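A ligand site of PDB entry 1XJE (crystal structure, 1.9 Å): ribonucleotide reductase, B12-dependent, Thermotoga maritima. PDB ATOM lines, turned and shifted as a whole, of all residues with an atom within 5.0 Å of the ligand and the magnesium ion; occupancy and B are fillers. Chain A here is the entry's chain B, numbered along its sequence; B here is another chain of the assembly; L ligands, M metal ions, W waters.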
ATOM      1  N   ASP A 141      19.790 -19.758 -11.729  1.00  0.00           N
ATOM      2  CA  ASP A 141      19.660 -18.599 -10.867  1.00  0.00           C
ATOM      3  C   ASP A 141      20.905 -18.344 -10.020  1.00  0.00           C
ATOM      4  O   ASP A 141      20.794 -18.325  -8.783  1.00  0.00           O
ATOM      5  CB  ASP A 141      18.455 -18.878  -9.931  1.00  0.00           C
ATOM      6  CG  ASP A 141      18.026 -17.681  -9.136  1.00  0.00           C
ATOM      7  OD1 ASP A 141      18.196 -16.531  -9.583  1.00  0.00           O
ATOM      8  OD2 ASP A 141      17.498 -17.909  -7.998  1.00  0.00           O
ATOM      9  N   SER A 142      22.073 -18.168 -10.655  1.00  0.00           N
ATOM     10  CA  SER A 142      23.329 -17.771  -9.987  1.00  0.00           C
ATOM     11  C   SER A 142      24.241 -17.005 -10.934  1.00  0.00           C
ATOM     12  O   SER A 142      24.112 -17.148 -12.156  1.00  0.00           O
ATOM     13  CB  SER A 142      24.094 -18.989  -9.489  1.00  0.00           C
ATOM     14  OG  SER A 142      24.615 -19.825 -10.537  1.00  0.00           O
ATOM     15  N   ILE A 143      25.160 -16.217 -10.379  1.00  0.00           N
ATOM     16  CA  ILE A 143      26.095 -15.424 -11.209  1.00  0.00           C
ATOM     17  C   ILE A 143      26.939 -16.361 -12.058  1.00  0.00           C
ATOM     18  O   ILE A 143      27.134 -16.135 -13.256  1.00  0.00           O
ATOM     19  CB  ILE A 143      26.978 -14.443 -10.314  1.00  0.00           C
ATOM     20  CG1 ILE A 143      26.115 -13.368  -9.687  1.00  0.00           C
ATOM     21  CG2 ILE A 143      28.140 -13.782 -11.105  1.00  0.00           C
ATOM     22  CD1 ILE A 143      25.413 -12.391 -10.643  1.00  0.00           C
ATOM     23  N   GLU A 144      27.430 -17.458 -11.468  1.00  0.00           N
ATOM     24  CA  GLU A 144      28.162 -18.458 -12.251  1.00  0.00           C
ATOM     25  C   GLU A 144      27.397 -18.872 -13.509  1.00  0.00           C
ATOM     26  O   GLU A 144      27.921 -18.855 -14.615  1.00  0.00           O
ATOM     27  CB  GLU A 144      28.439 -19.703 -11.394  1.00  0.00           C
ATOM     28  CG  GLU A 144      28.868 -20.933 -12.164  1.00  0.00           C
ATOM     29  CD  GLU A 144      30.228 -20.830 -12.801  1.00  0.00           C
ATOM     30  OE1 GLU A 144      31.158 -20.322 -12.104  1.00  0.00           O
ATOM     31  OE2 GLU A 144      30.384 -21.274 -13.990  1.00  0.00           O
ATOM     32  N   ILE A 146      24.485 -17.614 -14.955  1.00  0.00           N
ATOM     33  CA  ILE A 146      24.165 -16.491 -15.891  1.00  0.00           C
ATOM     34  C   ILE A 146      25.326 -16.211 -16.856  1.00  0.00           C
ATOM     35  O   ILE A 146      25.148 -16.201 -18.059  1.00  0.00           O
ATOM     36  CB  ILE A 146      23.784 -15.219 -15.127  1.00  0.00           C
ATOM     37  CG1 ILE A 146      22.442 -15.448 -14.391  1.00  0.00           C
ATOM     38  CG2 ILE A 146      23.776 -13.982 -16.016  1.00  0.00           C
ATOM     39  CD1 ILE A 146      22.188 -14.408 -13.369  1.00  0.00           C
ATOM     40  N   LEU A 170      15.574 -16.980 -12.944  1.00  0.00           N
ATOM     41  CA  LEU A 170      16.204 -15.864 -12.275  1.00  0.00           C
ATOM     42  C   LEU A 170      15.200 -15.202 -11.326  1.00  0.00           C
ATOM     43  O   LEU A 170      14.082 -14.878 -11.686  1.00  0.00           O
ATOM     44  CB  LEU A 170      16.704 -14.840 -13.253  1.00  0.00           C
ATOM     45  CG  LEU A 170      17.684 -15.408 -14.268  1.00  0.00           C
ATOM     46  CD1 LEU A 170      18.279 -14.183 -15.052  1.00  0.00           C
ATOM     47  CD2 LEU A 170      18.718 -16.251 -13.658  1.00  0.00           C
ATOM     48  N   ARG A 171      15.633 -14.994 -10.108  1.00  0.00           N
ATOM     49  CA  ARG A 171      14.703 -14.542  -9.063  1.00  0.00           C
ATOM     50  C   ARG A 171      14.386 -13.122  -9.374  1.00  0.00           C
ATOM     51  O   ARG A 171      15.206 -12.408  -9.990  1.00  0.00           O
ATOM     52  CB  ARG A 171      15.311 -14.748  -7.670  1.00  0.00           C
ATOM     53  CG  ARG A 171      16.542 -13.902  -7.400  1.00  0.00           C
ATOM     54  CD  ARG A 171      17.255 -14.314  -6.128  1.00  0.00           C
ATOM     55  NE  ARG A 171      17.755 -15.678  -6.202  1.00  0.00           N
ATOM     56  CZ  ARG A 171      18.531 -16.231  -5.302  1.00  0.00           C
ATOM     57  NH1 ARG A 171      18.895 -15.507  -4.242  1.00  0.00           N
ATOM     58  NH2 ARG A 171      18.973 -17.489  -5.440  1.00  0.00           N
ATOM     59  N   PHE A 176      15.936 -11.321  -2.203  1.00  0.00           N
ATOM     60  CA  PHE A 176      17.085 -11.331  -1.328  1.00  0.00           C
ATOM     61  C   PHE A 176      18.136 -12.161  -2.015  1.00  0.00           C
ATOM     62  O   PHE A 176      17.820 -13.223  -2.529  1.00  0.00           O
ATOM     63  CB  PHE A 176      16.703 -11.927   0.030  1.00  0.00           C
ATOM     64  CG  PHE A 176      17.805 -11.874   1.071  1.00  0.00           C
ATOM     65  CD1 PHE A 176      18.316 -13.038   1.616  1.00  0.00           C
ATOM     66  CD2 PHE A 176      18.268 -10.667   1.543  1.00  0.00           C
ATOM     67  CE1 PHE A 176      19.311 -12.996   2.595  1.00  0.00           C
ATOM     68  CE2 PHE A 176      19.270 -10.608   2.539  1.00  0.00           C
ATOM     69  CZ  PHE A 176      19.787 -11.783   3.050  1.00  0.00           C
ATOM     70  N   VAL A 177      19.358 -11.683  -1.975  1.00  0.00           N
ATOM     71  CA  VAL A 177      20.536 -12.471  -2.343  1.00  0.00           C
ATOM     72  C   VAL A 177      21.340 -12.782  -1.084  1.00  0.00           C
ATOM     73  O   VAL A 177      22.053 -11.894  -0.535  1.00  0.00           O
ATOM     74  CB  VAL A 177      21.405 -11.713  -3.346  1.00  0.00           C
ATOM     75  CG1 VAL A 177      22.595 -12.551  -3.803  1.00  0.00           C
ATOM     76  CG2 VAL A 177      20.552 -11.233  -4.534  1.00  0.00           C
ATOM     77  N   ALA A 178      21.234 -14.024  -0.630  1.00  0.00           N
ATOM     78  CA  ALA A 178      21.784 -14.411   0.660  1.00  0.00           C
ATOM     79  C   ALA A 178      23.261 -14.154   0.692  1.00  0.00           C
ATOM     80  O   ALA A 178      23.810 -13.740   1.730  1.00  0.00           O
ATOM     81  CB  ALA A 178      21.506 -15.852   0.958  1.00  0.00           C
ATOM     82  N   GLY A 179      23.920 -14.393  -0.431  1.00  0.00           N
ATOM     83  CA  GLY A 179      25.376 -14.333  -0.491  1.00  0.00           C
ATOM     84  C   GLY A 179      25.947 -12.978  -0.217  1.00  0.00           C
ATOM     85  O   GLY A 179      27.053 -12.887   0.321  1.00  0.00           O
ATOM     86  N   THR A 180      25.221 -11.931  -0.564  1.00  0.00           N
ATOM     87  CA  THR A 180      25.684 -10.566  -0.418  1.00  0.00           C
ATOM     88  C   THR A 180      24.800  -9.730   0.510  1.00  0.00           C
ATOM     89  O   THR A 180      25.067  -8.542   0.702  1.00  0.00           O
ATOM     90  CB  THR A 180      25.641  -9.839  -1.781  1.00  0.00           C
ATOM     91  OG1 THR A 180      24.294  -9.828  -2.288  1.00  0.00           O
ATOM     92  CG2 THR A 180      26.558 -10.500  -2.788  1.00  0.00           C
ATOM     93  N   LYS A 183      20.008  -7.073  -3.115  1.00  0.00           N
ATOM     94  CA  LYS A 183      18.736  -7.201  -3.795  1.00  0.00           C
ATOM     95  C   LYS A 183      19.015  -7.614  -5.249  1.00  0.00           C
ATOM     96  O   LYS A 183      19.855  -7.023  -5.923  1.00  0.00           O
ATOM     97  CB  LYS A 183      17.939  -5.909  -3.737  1.00  0.00           C
ATOM     98  CG  LYS A 183      17.759  -5.311  -2.299  1.00  0.00           C
ATOM     99  CD  LYS A 183      16.531  -5.768  -1.521  1.00  0.00           C
ATOM    100  CE  LYS A 183      16.062  -4.617  -0.606  1.00  0.00           C
ATOM    101  NZ  LYS A 183      14.950  -4.996   0.309  1.00  0.00           N
ATOM    102  N   ALA A 184      18.317  -8.636  -5.725  1.00  0.00           N
ATOM    103  CA  ALA A 184      18.577  -9.158  -7.092  1.00  0.00           C
ATOM    104  C   ALA A 184      18.170  -8.130  -8.129  1.00  0.00           C
ATOM    105  O   ALA A 184      17.201  -7.434  -7.958  1.00  0.00           O
ATOM    106  CB  ALA A 184      17.836 -10.416  -7.320  1.00  0.00           C
ATOM    107  N   SER A 185      18.877  -8.108  -9.256  1.00  0.00           N
ATOM    108  CA  SER A 185      18.555  -7.201 -10.345  1.00  0.00           C
ATOM    109  C   SER A 185      17.339  -7.659 -11.172  1.00  0.00           C
ATOM    110  O   SER A 185      16.735  -6.867 -11.855  1.00  0.00           O
ATOM    111  CB  SER A 185      19.781  -7.062 -11.259  1.00  0.00           C
ATOM    112  OG  SER A 185      20.916  -6.502 -10.604  1.00  0.00           O
ATOM    113  N   GLY A 186      17.062  -8.961 -11.193  1.00  0.00           N
ATOM    114  CA  GLY A 186      15.940  -9.523 -11.921  1.00  0.00           C
ATOM    115  C   GLY A 186      16.297  -9.963 -13.331  1.00  0.00           C
ATOM    116  O   GLY A 186      17.303  -9.534 -13.859  1.00  0.00           O
ATOM    117  N   PHE A 190      19.365  -8.639 -16.435  1.00  0.00           N
ATOM    118  CA  PHE A 190      20.277  -9.614 -17.013  1.00  0.00           C
ATOM    119  C   PHE A 190      20.179  -9.878 -18.516  1.00  0.00           C
ATOM    120  O   PHE A 190      21.207 -10.027 -19.177  1.00  0.00           O
ATOM    121  CB  PHE A 190      20.213 -10.894 -16.258  1.00  0.00           C
ATOM    122  CG  PHE A 190      20.881 -10.808 -14.967  1.00  0.00           C
ATOM    123  CD1 PHE A 190      22.239 -10.591 -14.927  1.00  0.00           C
ATOM    124  CD2 PHE A 190      20.162 -10.909 -13.756  1.00  0.00           C
ATOM    125  CE1 PHE A 190      22.905 -10.512 -13.694  1.00  0.00           C
ATOM    126  CE2 PHE A 190      20.822 -10.795 -12.511  1.00  0.00           C
ATOM    127  CZ  PHE A 190      22.193 -10.596 -12.495  1.00  0.00           C
ATOM    128  N   HIS B 127      32.419 -20.285   0.233  1.00  0.00           N
ATOM    129  CA  HIS B 127      33.002 -19.818  -1.012  1.00  0.00           C
ATOM    130  C   HIS B 127      33.012 -18.274  -1.176  1.00  0.00           C
ATOM    131  O   HIS B 127      33.557 -17.725  -2.165  1.00  0.00           O
ATOM    132  CB  HIS B 127      32.261 -20.491  -2.194  1.00  0.00           C
ATOM    133  CG  HIS B 127      30.814 -20.079  -2.302  1.00  0.00           C
ATOM    134  ND1 HIS B 127      29.901 -20.313  -1.303  1.00  0.00           N
ATOM    135  CD2 HIS B 127      30.148 -19.429  -3.295  1.00  0.00           C
ATOM    136  CE1 HIS B 127      28.717 -19.823  -1.664  1.00  0.00           C
ATOM    137  NE2 HIS B 127      28.840 -19.286  -2.872  1.00  0.00           N
ATOM    138  N   LEU B 128      32.376 -17.577  -0.230  1.00  0.00           N
ATOM    139  CA  LEU B 128      32.292 -16.127  -0.228  1.00  0.00           C
ATOM    140  C   LEU B 128      33.284 -15.505   0.758  1.00  0.00           C
ATOM    141  O   LEU B 128      33.247 -14.287   0.983  1.00  0.00           O
ATOM    142  CB  LEU B 128      30.919 -15.713   0.190  1.00  0.00           C
ATOM    143  CG  LEU B 128      29.844 -16.301  -0.686  1.00  0.00           C
ATOM    144  CD1 LEU B 128      28.547 -16.059  -0.020  1.00  0.00           C
ATOM    145  CD2 LEU B 128      29.865 -15.685  -2.036  1.00  0.00           C
ATOM    146  N   LYS B 158      31.225  -9.891  -7.123  1.00  0.00           N
ATOM    147  CA  LYS B 158      30.220 -10.400  -6.190  1.00  0.00           C
ATOM    148  C   LYS B 158      30.757 -10.453  -4.741  1.00  0.00           C
ATOM    149  O   LYS B 158      30.074 -10.142  -3.752  1.00  0.00           O
ATOM    150  CB  LYS B 158      29.800 -11.806  -6.659  1.00  0.00           C
ATOM    151  CG  LYS B 158      28.990 -12.674  -5.607  1.00  0.00           C
ATOM    152  CD  LYS B 158      28.519 -13.915  -6.150  1.00  0.00           C
ATOM    153  CE  LYS B 158      27.773 -14.716  -5.024  1.00  0.00           C
ATOM    154  NZ  LYS B 158      27.242 -15.850  -5.689  1.00  0.00           N
ATOM    155  N   VAL B 200      25.235  -4.855 -13.269  1.00  0.00           N
ATOM    156  CA  VAL B 200      24.248  -5.737 -12.582  1.00  0.00           C
ATOM    157  C   VAL B 200      24.832  -6.663 -11.498  1.00  0.00           C
ATOM    158  O   VAL B 200      24.179  -7.617 -11.076  1.00  0.00           O
ATOM    159  CB  VAL B 200      23.497  -6.659 -13.594  1.00  0.00           C
ATOM    160  CG1 VAL B 200      22.796  -5.828 -14.577  1.00  0.00           C
ATOM    161  CG2 VAL B 200      24.462  -7.581 -14.399  1.00  0.00           C
ATOM    162  N   VAL B 201      26.076  -6.436 -11.096  1.00  0.00           N
ATOM    163  CA  VAL B 201      26.708  -7.255 -10.070  1.00  0.00           C
ATOM    164  C   VAL B 201      27.339  -6.308  -9.012  1.00  0.00           C
ATOM    165  O   VAL B 201      27.979  -5.320  -9.326  1.00  0.00           O
ATOM    166  CB  VAL B 201      27.805  -8.158 -10.630  1.00  0.00           C
ATOM    167  CG1 VAL B 201      28.338  -9.082  -9.569  1.00  0.00           C
ATOM    168  CG2 VAL B 201      27.312  -8.959 -11.827  1.00  0.00           C
ATOM    169  N   LYS B 202      27.166  -6.660  -7.751  1.00  0.00           N
ATOM    170  CA  LYS B 202      27.777  -5.904  -6.697  1.00  0.00           C
ATOM    171  C   LYS B 202      27.784  -6.740  -5.410  1.00  0.00           C
ATOM    172  O   LYS B 202      27.119  -7.785  -5.337  1.00  0.00           O
ATOM    173  CB  LYS B 202      27.039  -4.565  -6.492  1.00  0.00           C
ATOM    174  CG  LYS B 202      25.522  -4.653  -6.355  1.00  0.00           C
ATOM    175  CD  LYS B 202      25.006  -3.282  -5.963  1.00  0.00           C
ATOM    176  CE  LYS B 202      23.511  -3.276  -5.731  1.00  0.00           C
ATOM    177  NZ  LYS B 202      23.033  -1.860  -5.592  1.00  0.00           N
HETATM  178  P1  LIG L   1      24.062 -15.908  -6.707  1.00  0.00           P
HETATM  179  O1  LIG L   1      23.534 -17.237  -6.508  1.00  0.00           O
HETATM  180  O2  LIG L   1      25.342 -15.814  -7.436  1.00  0.00           O
HETATM  181  O3  LIG L   1      24.138 -15.321  -5.181  1.00  0.00           O
HETATM  182  P2  LIG L   1      24.305 -16.392  -3.747  1.00  0.00           P
HETATM  183  O4  LIG L   1      25.490 -15.922  -3.013  1.00  0.00           O
HETATM  184  O5  LIG L   1      24.262 -17.872  -4.101  1.00  0.00           O
HETATM  185  O6  LIG L   1      23.017 -16.015  -2.924  1.00  0.00           O
HETATM  186  P3  LIG L   1      21.838 -17.128  -2.753  1.00  0.00           P
HETATM  187  O7  LIG L   1      20.752 -16.410  -2.021  1.00  0.00           O
HETATM  188  O8  LIG L   1      21.602 -17.685  -4.115  1.00  0.00           O
HETATM  189  O9  LIG L   1      22.398 -18.344  -1.851  1.00  0.00           O
HETATM  190  O10 LIG L   1      22.898 -15.226  -7.486  1.00  0.00           O
HETATM  191  C1  LIG L   1      21.548 -15.375  -7.087  1.00  0.00           C
HETATM  192  C2  LIG L   1      20.643 -14.531  -7.990  1.00  0.00           C
HETATM  193  O11 LIG L   1      20.886 -13.221  -7.554  1.00  0.00           O
HETATM  194  C3  LIG L   1      20.876 -14.550  -9.526  1.00  0.00           C
HETATM  195  O12 LIG L   1      19.644 -14.294 -10.255  1.00  0.00           O
HETATM  196  C4  LIG L   1      21.750 -13.290  -9.687  1.00  0.00           C
HETATM  197  C5  LIG L   1      21.150 -12.305  -8.664  1.00  0.00           C
HETATM  198  N1  LIG L   1      22.200 -11.363  -8.288  1.00  0.00           N
HETATM  199  C6  LIG L   1      22.171 -10.055  -8.694  1.00  0.00           C
HETATM  200  O13 LIG L   1      21.223  -9.625  -9.351  1.00  0.00           O
HETATM  201  N2  LIG L   1      23.150  -9.245  -8.333  1.00  0.00           N
HETATM  202  C7  LIG L   1      24.206  -9.679  -7.595  1.00  0.00           C
HETATM  203  O14 LIG L   1      25.186  -8.851  -7.211  1.00  0.00           O
HETATM  204  C8  LIG L   1      24.278 -10.974  -7.149  1.00  0.00           C
HETATM  205  C9  LIG L   1      25.355 -11.359  -6.361  1.00  0.00           C
HETATM  206  C10 LIG L   1      23.277 -11.842  -7.528  1.00  0.00           C
HETATM  207 MG    MG M   1      23.943 -18.861  -5.530  1.00  0.00          MG
HETATM  208  O   HOH W   1      22.660  -6.616  -8.570  1.00  0.00           O
HETATM  209  O   HOH W   2      27.551 -17.843  -8.560  1.00  0.00           O
HETATM  210  O   HOH W   3      18.053 -11.945 -10.412  1.00  0.00           O
HETATM  211  O   HOH W   4      24.472  -8.257  -4.462  1.00  0.00           O
HETATM  212  O   HOH W   5      17.868 -17.002  -0.955  1.00  0.00           O
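The magnesium ion is bound by O5 of the ligand (1.8 Å) and O1 of the ligand (1.9 Å).
Water W1 lies within hydrogen-bond range of the side-chain hydroxyl (OG) of Ser 185, a nitrogen (N2) of the ligand and the backbone carbonyl oxygen (O) of Val 200 of chain B. Water W3 lies within hydrogen-bond range of an oxygen (O12) of the ligand (2.8 Å), the backbone carbonyl oxygen of Arg 171 (2.9 Å) and the backbone NH of Gly 186 (3.2 Å). Water W4 lies within hydrogen-bond range of OG1 of Thr 180 (2.7 Å), O of Lys 202 of chain B (2.8 Å) and O14 of the ligand (2.9 Å). Water W2 lies within hydrogen-bond range of N of Glu 144, O2 of the ligand and N of Ile 143.
CB of Ser 142 touches the magnesium ion, 3.96 Å away. Of the 23 residues printed, 1 comes within 4 Å of the magnesium ion. The nearest printed residue that does not touch the magnesium ion is Lys 158 of chain B (4.5 Å).
NH2 of Arg 171 lies within salt-bridge range of O8 of the ligand, at 3.0 Å. An oxygen (O7) of the ligand sits at hydrogen-bond distance from the backbone NH (N) of Ala 178, at 2.8 Å. The backbone NH (N) of Ser 185 is in hydrogen-bond range of an oxygen (O13) of the ligand, 2.8 Å away. The backbone NH (N) of Lys 202 of chain B sits at hydrogen-bond distance from an oxygen (O14) of the ligand, 3.0 Å away. The side-chain amino group (NZ) of Lys 158 of chain B is in salt-bridge range of an oxygen (O2) of the ligand, 2.6 Å away. An oxygen (O2) of the ligand is in hydrogen-bond range of the backbone NH (N) of Ile 143, at 3.0 Å. An oxygen (O12) of the ligand is in hydrogen-bond range of the side-chain carboxylate (OD1) of Asp 141. OG of Ser 185 sits at hydrogen-bond distance from O13 of the ligand (3.4 Å). N2 of the ligand sits at hydrogen-bond distance from O of Val 200 of chain B (3.4 Å). N of Gly 179 sits at hydrogen-bond distance from O6 of the ligand (3.1 Å).
Ser 142 touches the ligand (CB to O1, 3.5 Å). Ile 146 touches the ligand. Val 177 touches the ligand (CG1 to O3, 3.5 Å). Thr 180 touches the ligand. CA of Ala 184 touches O13 of the ligand, at 3.5 Å. CE2 of Phe 190 touches O13 of the ligand (3.4 Å). Val 201 of chain B touches the ligand (CA to O14, 3.6 Å). Hydrophobic or aromatic side chains within 4 Å of the ligand: Ile 143, Ile 146, Val 177, Ala 178, Phe 190 and Val 201 of chain B. 16 residues have an atom within 4 Å of the ligand: Asp 141, Ser 142, Ile 143, Ile 146, Arg 171, Val 177, Ala 178, Gly 179, Thr 180, Ala 184, Ser 185, Phe 190, Lys 158 of chain B, Val 200 of chain B, Val 201 of chain B and Lys 202 of chain B.
The backbone carbonyl oxygen (O) of Val 200 of chain B is in hydrogen-bond range of the side-chain hydroxyl (OG) of Ser 185, at 3.5 Å. The side-chain carboxylate of Asp 141 is in salt-bridge range of the guanidinium group of Arg 171, at 2.9 Å. NH1 of Arg 171 lies within hydrogen-bond range of O of Phe 176 (3.1 Å).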
